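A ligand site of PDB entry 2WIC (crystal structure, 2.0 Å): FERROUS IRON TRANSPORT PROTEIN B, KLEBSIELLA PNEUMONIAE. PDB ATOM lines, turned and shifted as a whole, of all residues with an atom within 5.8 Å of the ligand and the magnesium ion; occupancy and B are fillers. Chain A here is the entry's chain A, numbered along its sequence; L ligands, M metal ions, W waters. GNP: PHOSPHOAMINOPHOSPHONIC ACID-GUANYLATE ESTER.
One residue has an atom within 4 Å of the magnesium ion: Thr 17.
Asn 11 touches the ligand.
Pro 12 touches the ligand (CA to O1G, 3.3 Å).
Gly 59 touches the ligand (N to O1G, 3.8 Å).
Ile 124 touches the ligand.
Val 149 touches the ligand (CA to O6, 3.5 Å).
Thr 151 touches the ligand (CG2 to O2', 3.5 Å).
Within 4 Å of the ligand: Asn 11, Pro 12, Asn 13, Ser 14, Gly 15, Lys 16, Thr 17, Thr 18, Gly 59, Asn 120, Met 121, Asp 123, Ile 124, Val 149, Ser 150 and Thr 151.
The nearest printed residue that does not touch the ligand is Leu 148 (4.4 Å).
The side-chain hydroxyl (OG1) of Thr 17 lies close to the side-chain carboxylate (OD2) of Asp 56, at 2.7 Å.
O of Ser 14 lies close to OD1 of Asn 120, at 3.0 Å.
The side-chain amide nitrogen of Asn 120 sits at hydrogen-bond distance from the side-chain hydroxyl of Ser 150 (2.8 Å).
The backbone carbonyl oxygen (O) of Gly 59 sits at hydrogen-bond distance from the backbone NH (N) of Asp 73 (3.1 Å).
The side-chain amino group (NZ) of Lys 16 lies within hydrogen-bond range of the backbone carbonyl oxygen (O) of Asn 11 (3.0 Å).
NH2 of Arg 152 is in salt-bridge range of OD2 of Asp 123 (3.6 Å).
OG of Ser 14 lies within hydrogen-bond range of O of Asn 11, 2.8 Å away.
N of Lys 16 lies within hydrogen-bond range of O2B of the ligand (3.0 Å).
N of Gly 15 lies within hydrogen-bond range of O2B of the ligand, 2.8 Å away.
The backbone NH (N) of Thr 17 lies within hydrogen-bond range of an oxygen (O1A) of the ligand.
The side-chain amino group (NZ) of Lys 16 lies within salt-bridge range of an oxygen (O2B) of the ligand.
An oxygen (O2B) of the ligand lies within hydrogen-bond range of the backbone NH (N) of Ser 14 (2.7 Å).
The backbone NH (N) of Asn 13 lies within hydrogen-bond range of an oxygen (O2B) of the ligand, at 3.4 Å.
The backbone NH of Met 121 sits at hydrogen-bond distance from an oxygen (O6) of the ligand (3.1 Å).
An oxygen (O1A) of the ligand lies within hydrogen-bond range of the backbone NH (N) of Thr 18 (2.7 Å).
N of Ser 150 sits at hydrogen-bond distance from O6 of the ligand.
A nitrogen (N2) of the ligand lies within hydrogen-bond range of the side-chain carboxylate (OD2) of Asp 123, 2.6 Å away.
OG1 of Thr 18 is in hydrogen-bond range of O1A of the ligand (2.5 Å).
The side-chain amide oxygen (OD1) of Asn 120 lies close to a nitrogen (N7) of the ligand (3.0 Å).
The magnesium ion is bound by water W3 (2.0 Å), water W1 (2.0 Å), water W2 (2.1 Å), O2G of the ligand (2.1 Å), O1B of the ligand (2.1 Å) and OG1 of Thr 17 (2.1 Å).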
ATOM      1  N   GLY A  10       1.211  29.306  18.242  1.00  0.00           N
ATOM      2  CA  GLY A  10       2.166  28.219  18.421  1.00  0.00           C
ATOM      3  C   GLY A  10       1.815  27.124  17.420  1.00  0.00           C
ATOM      4  O   GLY A  10       0.778  27.206  16.730  1.00  0.00           O
ATOM      5  N   ASN A  11       2.694  26.118  17.344  1.00  0.00           N
ATOM      6  CA  ASN A  11       2.474  24.958  16.492  1.00  0.00           C
ATOM      7  C   ASN A  11       1.213  24.228  16.955  1.00  0.00           C
ATOM      8  O   ASN A  11       0.831  24.335  18.138  1.00  0.00           O
ATOM      9  CB  ASN A  11       3.652  23.964  16.568  1.00  0.00           C
ATOM     10  CG  ASN A  11       4.968  24.534  16.026  1.00  0.00           C
ATOM     11  OD1 ASN A  11       5.030  25.616  15.448  1.00  0.00           O
ATOM     12  ND2 ASN A  11       6.023  23.783  16.213  1.00  0.00           N
ATOM     13  N   PRO A  12       0.595  23.433  16.038  1.00  0.00           N
ATOM     14  CA  PRO A  12      -0.458  22.493  16.468  1.00  0.00           C
ATOM     15  C   PRO A  12      -0.003  21.652  17.646  1.00  0.00           C
ATOM     16  O   PRO A  12       1.157  21.216  17.705  1.00  0.00           O
ATOM     17  CB  PRO A  12      -0.705  21.631  15.222  1.00  0.00           C
ATOM     18  CG  PRO A  12      -0.462  22.554  14.098  1.00  0.00           C
ATOM     19  CD  PRO A  12       0.794  23.374  14.566  1.00  0.00           C
ATOM     20  N   ASN A  13      -0.892  21.477  18.603  1.00  0.00           N
ATOM     21  CA  ASN A  13      -0.642  20.616  19.749  1.00  0.00           C
ATOM     22  C   ASN A  13       0.452  21.030  20.715  1.00  0.00           C
ATOM     23  O   ASN A  13       1.099  20.158  21.314  1.00  0.00           O
ATOM     24  CB  ASN A  13      -0.424  19.157  19.296  1.00  0.00           C
ATOM     25  CG  ASN A  13      -1.700  18.527  18.762  1.00  0.00           C
ATOM     26  OD1 ASN A  13      -1.762  18.148  17.585  1.00  0.00           O
ATOM     27  ND2 ASN A  13      -2.746  18.468  19.617  1.00  0.00           N
ATOM     28  N   SER A  14       0.587  22.343  20.948  1.00  0.00           N
ATOM     29  CA  SER A  14       1.701  22.848  21.777  1.00  0.00           C
ATOM     30  C   SER A  14       1.187  23.238  23.160  1.00  0.00           C
ATOM     31  O   SER A  14       1.963  23.524  24.067  1.00  0.00           O
ATOM     32  CB  SER A  14       2.398  24.027  21.066  1.00  0.00           C
ATOM     33  OG  SER A  14       1.468  25.065  20.736  1.00  0.00           O
ATOM     34  N   GLY A  15      -0.143  23.165  23.302  1.00  0.00           N
ATOM     35  CA  GLY A  15      -0.858  23.430  24.562  1.00  0.00           C
ATOM     36  C   GLY A  15      -1.556  24.786  24.600  1.00  0.00           C
ATOM     37  O   GLY A  15      -1.867  25.247  25.659  1.00  0.00           O
ATOM     38  N   LYS A  16      -1.806  25.431  23.462  1.00  0.00           N
ATOM     39  CA  LYS A  16      -2.431  26.795  23.477  1.00  0.00           C
ATOM     40  C   LYS A  16      -3.791  26.848  24.210  1.00  0.00           C
ATOM     41  O   LYS A  16      -4.054  27.697  25.095  1.00  0.00           O
ATOM     42  CB  LYS A  16      -2.601  27.291  22.058  1.00  0.00           C
ATOM     43  CG  LYS A  16      -1.271  27.341  21.204  1.00  0.00           C
ATOM     44  CD  LYS A  16      -1.533  27.853  19.800  1.00  0.00           C
ATOM     45  CE  LYS A  16      -2.402  26.880  18.990  1.00  0.00           C
ATOM     46  NZ  LYS A  16      -1.833  25.538  18.824  1.00  0.00           N
ATOM     47  N   THR A  17      -4.694  25.948  23.829  1.00  0.00           N
ATOM     48  CA  THR A  17      -6.020  25.920  24.458  1.00  0.00           C
ATOM     49  C   THR A  17      -5.970  25.579  25.936  1.00  0.00           C
ATOM     50  O   THR A  17      -6.693  26.178  26.719  1.00  0.00           O
ATOM     51  CB  THR A  17      -6.966  24.991  23.691  1.00  0.00           C
ATOM     52  OG1 THR A  17      -7.019  25.474  22.341  1.00  0.00           O
ATOM     53  CG2 THR A  17      -8.390  24.984  24.330  1.00  0.00           C
ATOM     54  N   THR A  18      -5.104  24.654  26.309  1.00  0.00           N
ATOM     55  CA  THR A  18      -4.893  24.333  27.704  1.00  0.00           C
ATOM     56  C   THR A  18      -4.492  25.593  28.475  1.00  0.00           C
ATOM     57  O   THR A  18      -5.048  25.905  29.551  1.00  0.00           O
ATOM     58  CB  THR A  18      -3.803  23.237  27.859  1.00  0.00           C
ATOM     59  OG1 THR A  18      -4.163  22.071  27.134  1.00  0.00           O
ATOM     60  CG2 THR A  18      -3.595  22.891  29.308  1.00  0.00           C
ATOM     61  N   LEU A  19      -3.494  26.295  27.948  1.00  0.00           N
ATOM     62  CA  LEU A  19      -3.059  27.560  28.569  1.00  0.00           C
ATOM     63  C   LEU A  19      -4.197  28.572  28.574  1.00  0.00           C
ATOM     64  O   LEU A  19      -4.427  29.254  29.588  1.00  0.00           O
ATOM     65  CB  LEU A  19      -1.874  28.134  27.781  1.00  0.00           C
ATOM     66  CG  LEU A  19      -1.283  29.459  28.349  1.00  0.00           C
ATOM     67  CD1 LEU A  19      -1.030  29.322  29.896  1.00  0.00           C
ATOM     68  CD2 LEU A  19       0.006  29.804  27.579  1.00  0.00           C
ATOM     69  N   ASP A  56      -7.242  32.736  21.366  1.00  0.00           N
ATOM     70  CA  ASP A  56      -6.681  31.418  21.104  1.00  0.00           C
ATOM     71  C   ASP A  56      -6.562  31.204  19.593  1.00  0.00           C
ATOM     72  O   ASP A  56      -7.521  30.896  18.960  1.00  0.00           O
ATOM     73  CB  ASP A  56      -7.576  30.357  21.799  1.00  0.00           C
ATOM     74  CG  ASP A  56      -7.037  28.927  21.712  1.00  0.00           C
ATOM     75  OD1 ASP A  56      -5.933  28.660  21.150  1.00  0.00           O
ATOM     76  OD2 ASP A  56      -7.752  28.023  22.252  1.00  0.00           O
ATOM     77  N   LEU A  57      -5.381  31.314  18.998  1.00  0.00           N
ATOM     78  CA  LEU A  57      -5.325  31.244  17.541  1.00  0.00           C
ATOM     79  C   LEU A  57      -5.061  29.812  17.059  1.00  0.00           C
ATOM     80  O   LEU A  57      -4.412  29.031  17.765  1.00  0.00           O
ATOM     81  CB  LEU A  57      -4.259  32.197  16.997  1.00  0.00           C
ATOM     82  CG  LEU A  57      -4.445  33.667  17.365  1.00  0.00           C
ATOM     83  CD1 LEU A  57      -3.194  34.428  17.000  1.00  0.00           C
ATOM     84  CD2 LEU A  57      -5.711  34.240  16.661  1.00  0.00           C
ATOM     85  N   PRO A  58      -5.590  29.440  15.860  1.00  0.00           N
ATOM     86  CA  PRO A  58      -5.300  28.100  15.253  1.00  0.00           C
ATOM     87  C   PRO A  58      -3.787  27.828  15.103  1.00  0.00           C
ATOM     88  O   PRO A  58      -3.036  28.733  14.705  1.00  0.00           O
ATOM     89  CB  PRO A  58      -5.973  28.219  13.880  1.00  0.00           C
ATOM     90  CG  PRO A  58      -7.176  29.164  14.158  1.00  0.00           C
ATOM     91  CD  PRO A  58      -6.546  30.223  15.045  1.00  0.00           C
ATOM     92  N   GLY A  59      -3.342  26.602  15.369  1.00  0.00           N
ATOM     93  CA  GLY A  59      -1.907  26.266  15.288  1.00  0.00           C
ATOM     94  C   GLY A  59      -1.337  26.390  13.903  1.00  0.00           C
ATOM     95  O   GLY A  59      -2.063  26.274  12.919  1.00  0.00           O
ATOM     96  N   ASP A  73      -4.718  24.747  12.360  1.00  0.00           N
ATOM     97  CA  ASP A  73      -5.683  24.899  11.263  1.00  0.00           C
ATOM     98  C   ASP A  73      -5.683  26.328  10.659  1.00  0.00           C
ATOM     99  O   ASP A  73      -6.736  26.982  10.615  1.00  0.00           O
ATOM    100  CB  ASP A  73      -7.105  24.515  11.746  1.00  0.00           C
ATOM    101  N   ASN A 120       6.251  25.421  27.238  1.00  0.00           N
ATOM    102  CA  ASN A 120       5.245  24.526  27.806  1.00  0.00           C
ATOM    103  C   ASN A 120       5.725  23.047  27.685  1.00  0.00           C
ATOM    104  O   ASN A 120       6.781  22.762  27.071  1.00  0.00           O
ATOM    105  CB  ASN A 120       3.928  24.703  27.010  1.00  0.00           C
ATOM    106  CG  ASN A 120       2.707  24.067  27.706  1.00  0.00           C
ATOM    107  OD1 ASN A 120       1.821  23.470  27.068  1.00  0.00           O
ATOM    108  ND2 ASN A 120       2.669  24.192  28.991  1.00  0.00           N
ATOM    109  N   MET A 121       4.957  22.112  28.259  1.00  0.00           N
ATOM    110  CA  MET A 121       5.282  20.688  28.214  1.00  0.00           C
ATOM    111  C   MET A 121       6.709  20.324  28.783  1.00  0.00           C
ATOM    112  O   MET A 121       7.392  19.409  28.272  1.00  0.00           O
ATOM    113  CB  MET A 121       5.137  20.186  26.793  1.00  0.00           C
ATOM    114  CG  MET A 121       3.712  20.273  26.224  1.00  0.00           C
ATOM    115  SD  MET A 121       3.417  19.787  24.517  1.00  0.00           S
ATOM    116  CE  MET A 121       1.622  20.071  24.648  1.00  0.00           C
ATOM    117  N   LEU A 122       7.134  21.054  29.815  1.00  0.00           N
ATOM    118  CA  LEU A 122       8.490  20.894  30.375  1.00  0.00           C
ATOM    119  C   LEU A 122       8.595  19.587  31.196  1.00  0.00           C
ATOM    120  O   LEU A 122       9.685  19.031  31.367  1.00  0.00           O
ATOM    121  CB  LEU A 122       8.934  22.097  31.204  1.00  0.00           C
ATOM    122  CG  LEU A 122       9.671  23.173  30.398  1.00  0.00           C
ATOM    123  CD1 LEU A 122       9.674  24.452  31.203  1.00  0.00           C
ATOM    124  CD2 LEU A 122      11.152  22.758  29.921  1.00  0.00           C
ATOM    125  N   ASP A 123       7.451  19.121  31.669  1.00  0.00           N
ATOM    126  CA  ASP A 123       7.328  17.759  32.265  1.00  0.00           C
ATOM    127  C   ASP A 123       7.629  16.651  31.244  1.00  0.00           C
ATOM    128  O   ASP A 123       8.326  15.718  31.572  1.00  0.00           O
ATOM    129  CB  ASP A 123       5.909  17.580  32.837  1.00  0.00           C
ATOM    130  CG  ASP A 123       4.825  17.691  31.787  1.00  0.00           C
ATOM    131  OD1 ASP A 123       4.796  18.645  30.970  1.00  0.00           O
ATOM    132  OD2 ASP A 123       3.965  16.815  31.769  1.00  0.00           O
ATOM    133  N   ILE A 124       7.120  16.769  30.025  1.00  0.00           N
ATOM    134  CA  ILE A 124       7.444  15.844  28.915  1.00  0.00           C
ATOM    135  C   ILE A 124       8.924  15.949  28.475  1.00  0.00           C
ATOM    136  O   ILE A 124       9.608  14.926  28.264  1.00  0.00           O
ATOM    137  CB  ILE A 124       6.601  16.133  27.658  1.00  0.00           C
ATOM    138  CG1 ILE A 124       5.117  16.095  27.985  1.00  0.00           C
ATOM    139  CG2 ILE A 124       6.980  15.146  26.495  1.00  0.00           C
ATOM    140  CD1 ILE A 124       4.243  16.388  26.768  1.00  0.00           C
ATOM    141  N   LEU A 148       6.496  26.550  31.710  1.00  0.00           N
ATOM    142  CA  LEU A 148       5.163  26.184  32.142  1.00  0.00           C
ATOM    143  C   LEU A 148       4.990  24.660  32.115  1.00  0.00           C
ATOM    144  O   LEU A 148       5.606  23.933  31.296  1.00  0.00           O
ATOM    145  CB  LEU A 148       4.083  26.725  31.180  1.00  0.00           C
ATOM    146  CG  LEU A 148       3.862  28.218  30.889  1.00  0.00           C
ATOM    147  CD1 LEU A 148       2.683  28.259  29.958  1.00  0.00           C
ATOM    148  CD2 LEU A 148       3.567  28.938  32.169  1.00  0.00           C
ATOM    149  N   VAL A 149       4.067  24.226  32.967  1.00  0.00           N
ATOM    150  CA  VAL A 149       3.382  22.969  32.749  1.00  0.00           C
ATOM    151  C   VAL A 149       1.900  23.344  32.834  1.00  0.00           C
ATOM    152  O   VAL A 149       1.351  23.444  33.914  1.00  0.00           O
ATOM    153  CB  VAL A 149       3.761  21.855  33.765  1.00  0.00           C
ATOM    154  CG1 VAL A 149       3.092  20.497  33.334  1.00  0.00           C
ATOM    155  CG2 VAL A 149       5.320  21.667  33.829  1.00  0.00           C
ATOM    156  N   SER A 150       1.306  23.604  31.673  1.00  0.00           N
ATOM    157  CA  SER A 150      -0.040  24.220  31.591  1.00  0.00           C
ATOM    158  C   SER A 150      -1.159  23.337  32.178  1.00  0.00           C
ATOM    159  O   SER A 150      -2.120  23.850  32.755  1.00  0.00           O
ATOM    160  CB  SER A 150      -0.352  24.607  30.160  1.00  0.00           C
ATOM    161  OG  SER A 150       0.450  25.748  29.788  1.00  0.00           O
ATOM    162  N   THR A 151      -1.009  22.018  32.059  1.00  0.00           N
ATOM    163  CA  THR A 151      -2.010  21.073  32.607  1.00  0.00           C
ATOM    164  C   THR A 151      -2.003  21.174  34.131  1.00  0.00           C
ATOM    165  O   THR A 151      -3.035  20.893  34.784  1.00  0.00           O
ATOM    166  CB  THR A 151      -1.714  19.614  32.153  1.00  0.00           C
ATOM    167  OG1 THR A 151      -0.306  19.376  32.201  1.00  0.00           O
ATOM    168  CG2 THR A 151      -2.211  19.364  30.739  1.00  0.00           C
ATOM    169  N   ARG A 152      -0.858  21.582  34.713  1.00  0.00           N
ATOM    170  CA  ARG A 152      -0.727  21.681  36.179  1.00  0.00           C
ATOM    171  C   ARG A 152      -0.893  23.118  36.695  1.00  0.00           C
ATOM    172  O   ARG A 152      -0.862  23.367  37.892  1.00  0.00           O
ATOM    173  CB  ARG A 152       0.609  21.076  36.654  1.00  0.00           C
ATOM    174  CG  ARG A 152       0.798  19.621  36.241  1.00  0.00           C
ATOM    175  CD  ARG A 152       1.970  18.939  36.988  1.00  0.00           C
ATOM    176  NE  ARG A 152       2.340  17.689  36.300  1.00  0.00           N
ATOM    177  CZ  ARG A 152       3.580  17.334  35.913  1.00  0.00           C
ATOM    178  NH1 ARG A 152       4.663  18.092  36.176  1.00  0.00           N
ATOM    179  NH2 ARG A 152       3.747  16.165  35.290  1.00  0.00           N
HETATM  180  PG  GNP L   1      -4.387  22.701  18.512  1.00  0.00           P
HETATM  181  O1G GNP L   1      -3.453  23.442  17.543  1.00  0.00           O
HETATM  182  O2G GNP L   1      -5.354  23.772  18.927  1.00  0.00           O
HETATM  183  O3G GNP L   1      -4.920  21.258  17.906  1.00  0.00           O
HETATM  184  N3B GNP L   1      -3.492  22.264  19.820  1.00  0.00           N
HETATM  185  PB  GNP L   1      -3.413  23.259  21.236  1.00  0.00           P
HETATM  186  O1B GNP L   1      -4.500  24.131  21.673  1.00  0.00           O
HETATM  187  O2B GNP L   1      -1.804  23.654  21.039  1.00  0.00           O
HETATM  188  O3A GNP L   1      -3.171  22.097  22.407  1.00  0.00           O
HETATM  189  PA  GNP L   1      -4.053  21.582  23.687  1.00  0.00           P
HETATM  190  O1A GNP L   1      -4.248  22.597  24.730  1.00  0.00           O
HETATM  191  O2A GNP L   1      -5.354  21.175  22.922  1.00  0.00           O
HETATM  192  O5' GNP L   1      -3.169  20.451  24.130  1.00  0.00           O
HETATM  193  C5' GNP L   1      -2.870  19.204  23.456  1.00  0.00           C
HETATM  194  C4' GNP L   1      -2.755  18.230  24.579  1.00  0.00           C
HETATM  195  O4' GNP L   1      -1.497  18.472  25.416  1.00  0.00           O
HETATM  196  C3' GNP L   1      -3.894  18.190  25.619  1.00  0.00           C
HETATM  197  O3' GNP L   1      -4.298  16.842  25.992  1.00  0.00           O
HETATM  198  C2' GNP L   1      -3.252  18.704  26.898  1.00  0.00           C
HETATM  199  O2' GNP L   1      -3.777  17.991  27.956  1.00  0.00           O
HETATM  200  C1' GNP L   1      -1.712  18.326  26.757  1.00  0.00           C
HETATM  201  N9  GNP L   1      -0.858  19.358  27.348  1.00  0.00           N
HETATM  202  C8  GNP L   1      -0.917  20.701  27.195  1.00  0.00           C
HETATM  203  N7  GNP L   1       0.026  21.292  27.981  1.00  0.00           N
HETATM  204  C5  GNP L   1       0.693  20.329  28.631  1.00  0.00           C
HETATM  205  C6  GNP L   1       1.842  20.256  29.381  1.00  0.00           C
HETATM  206  O6  GNP L   1       2.465  21.195  29.916  1.00  0.00           O
HETATM  207  N1  GNP L   1       2.261  18.935  29.789  1.00  0.00           N
HETATM  208  C2  GNP L   1       1.604  17.778  29.395  1.00  0.00           C
HETATM  209  N2  GNP L   1       2.109  16.632  29.892  1.00  0.00           N
HETATM  210  N3  GNP L   1       0.602  17.837  28.510  1.00  0.00           N
HETATM  211  C4  GNP L   1       0.119  19.094  28.171  1.00  0.00           C
HETATM  212 MG    MG M   1      -6.302  24.450  20.658  1.00  0.00          MG
HETATM  213  O   HOH W   1      -5.771  26.327  20.136  1.00  0.00           O
HETATM  214  O   HOH W   2      -8.111  24.861  19.778  1.00  0.00           O
HETATM  215  O   HOH W   3      -7.016  22.713  21.372  1.00  0.00           O
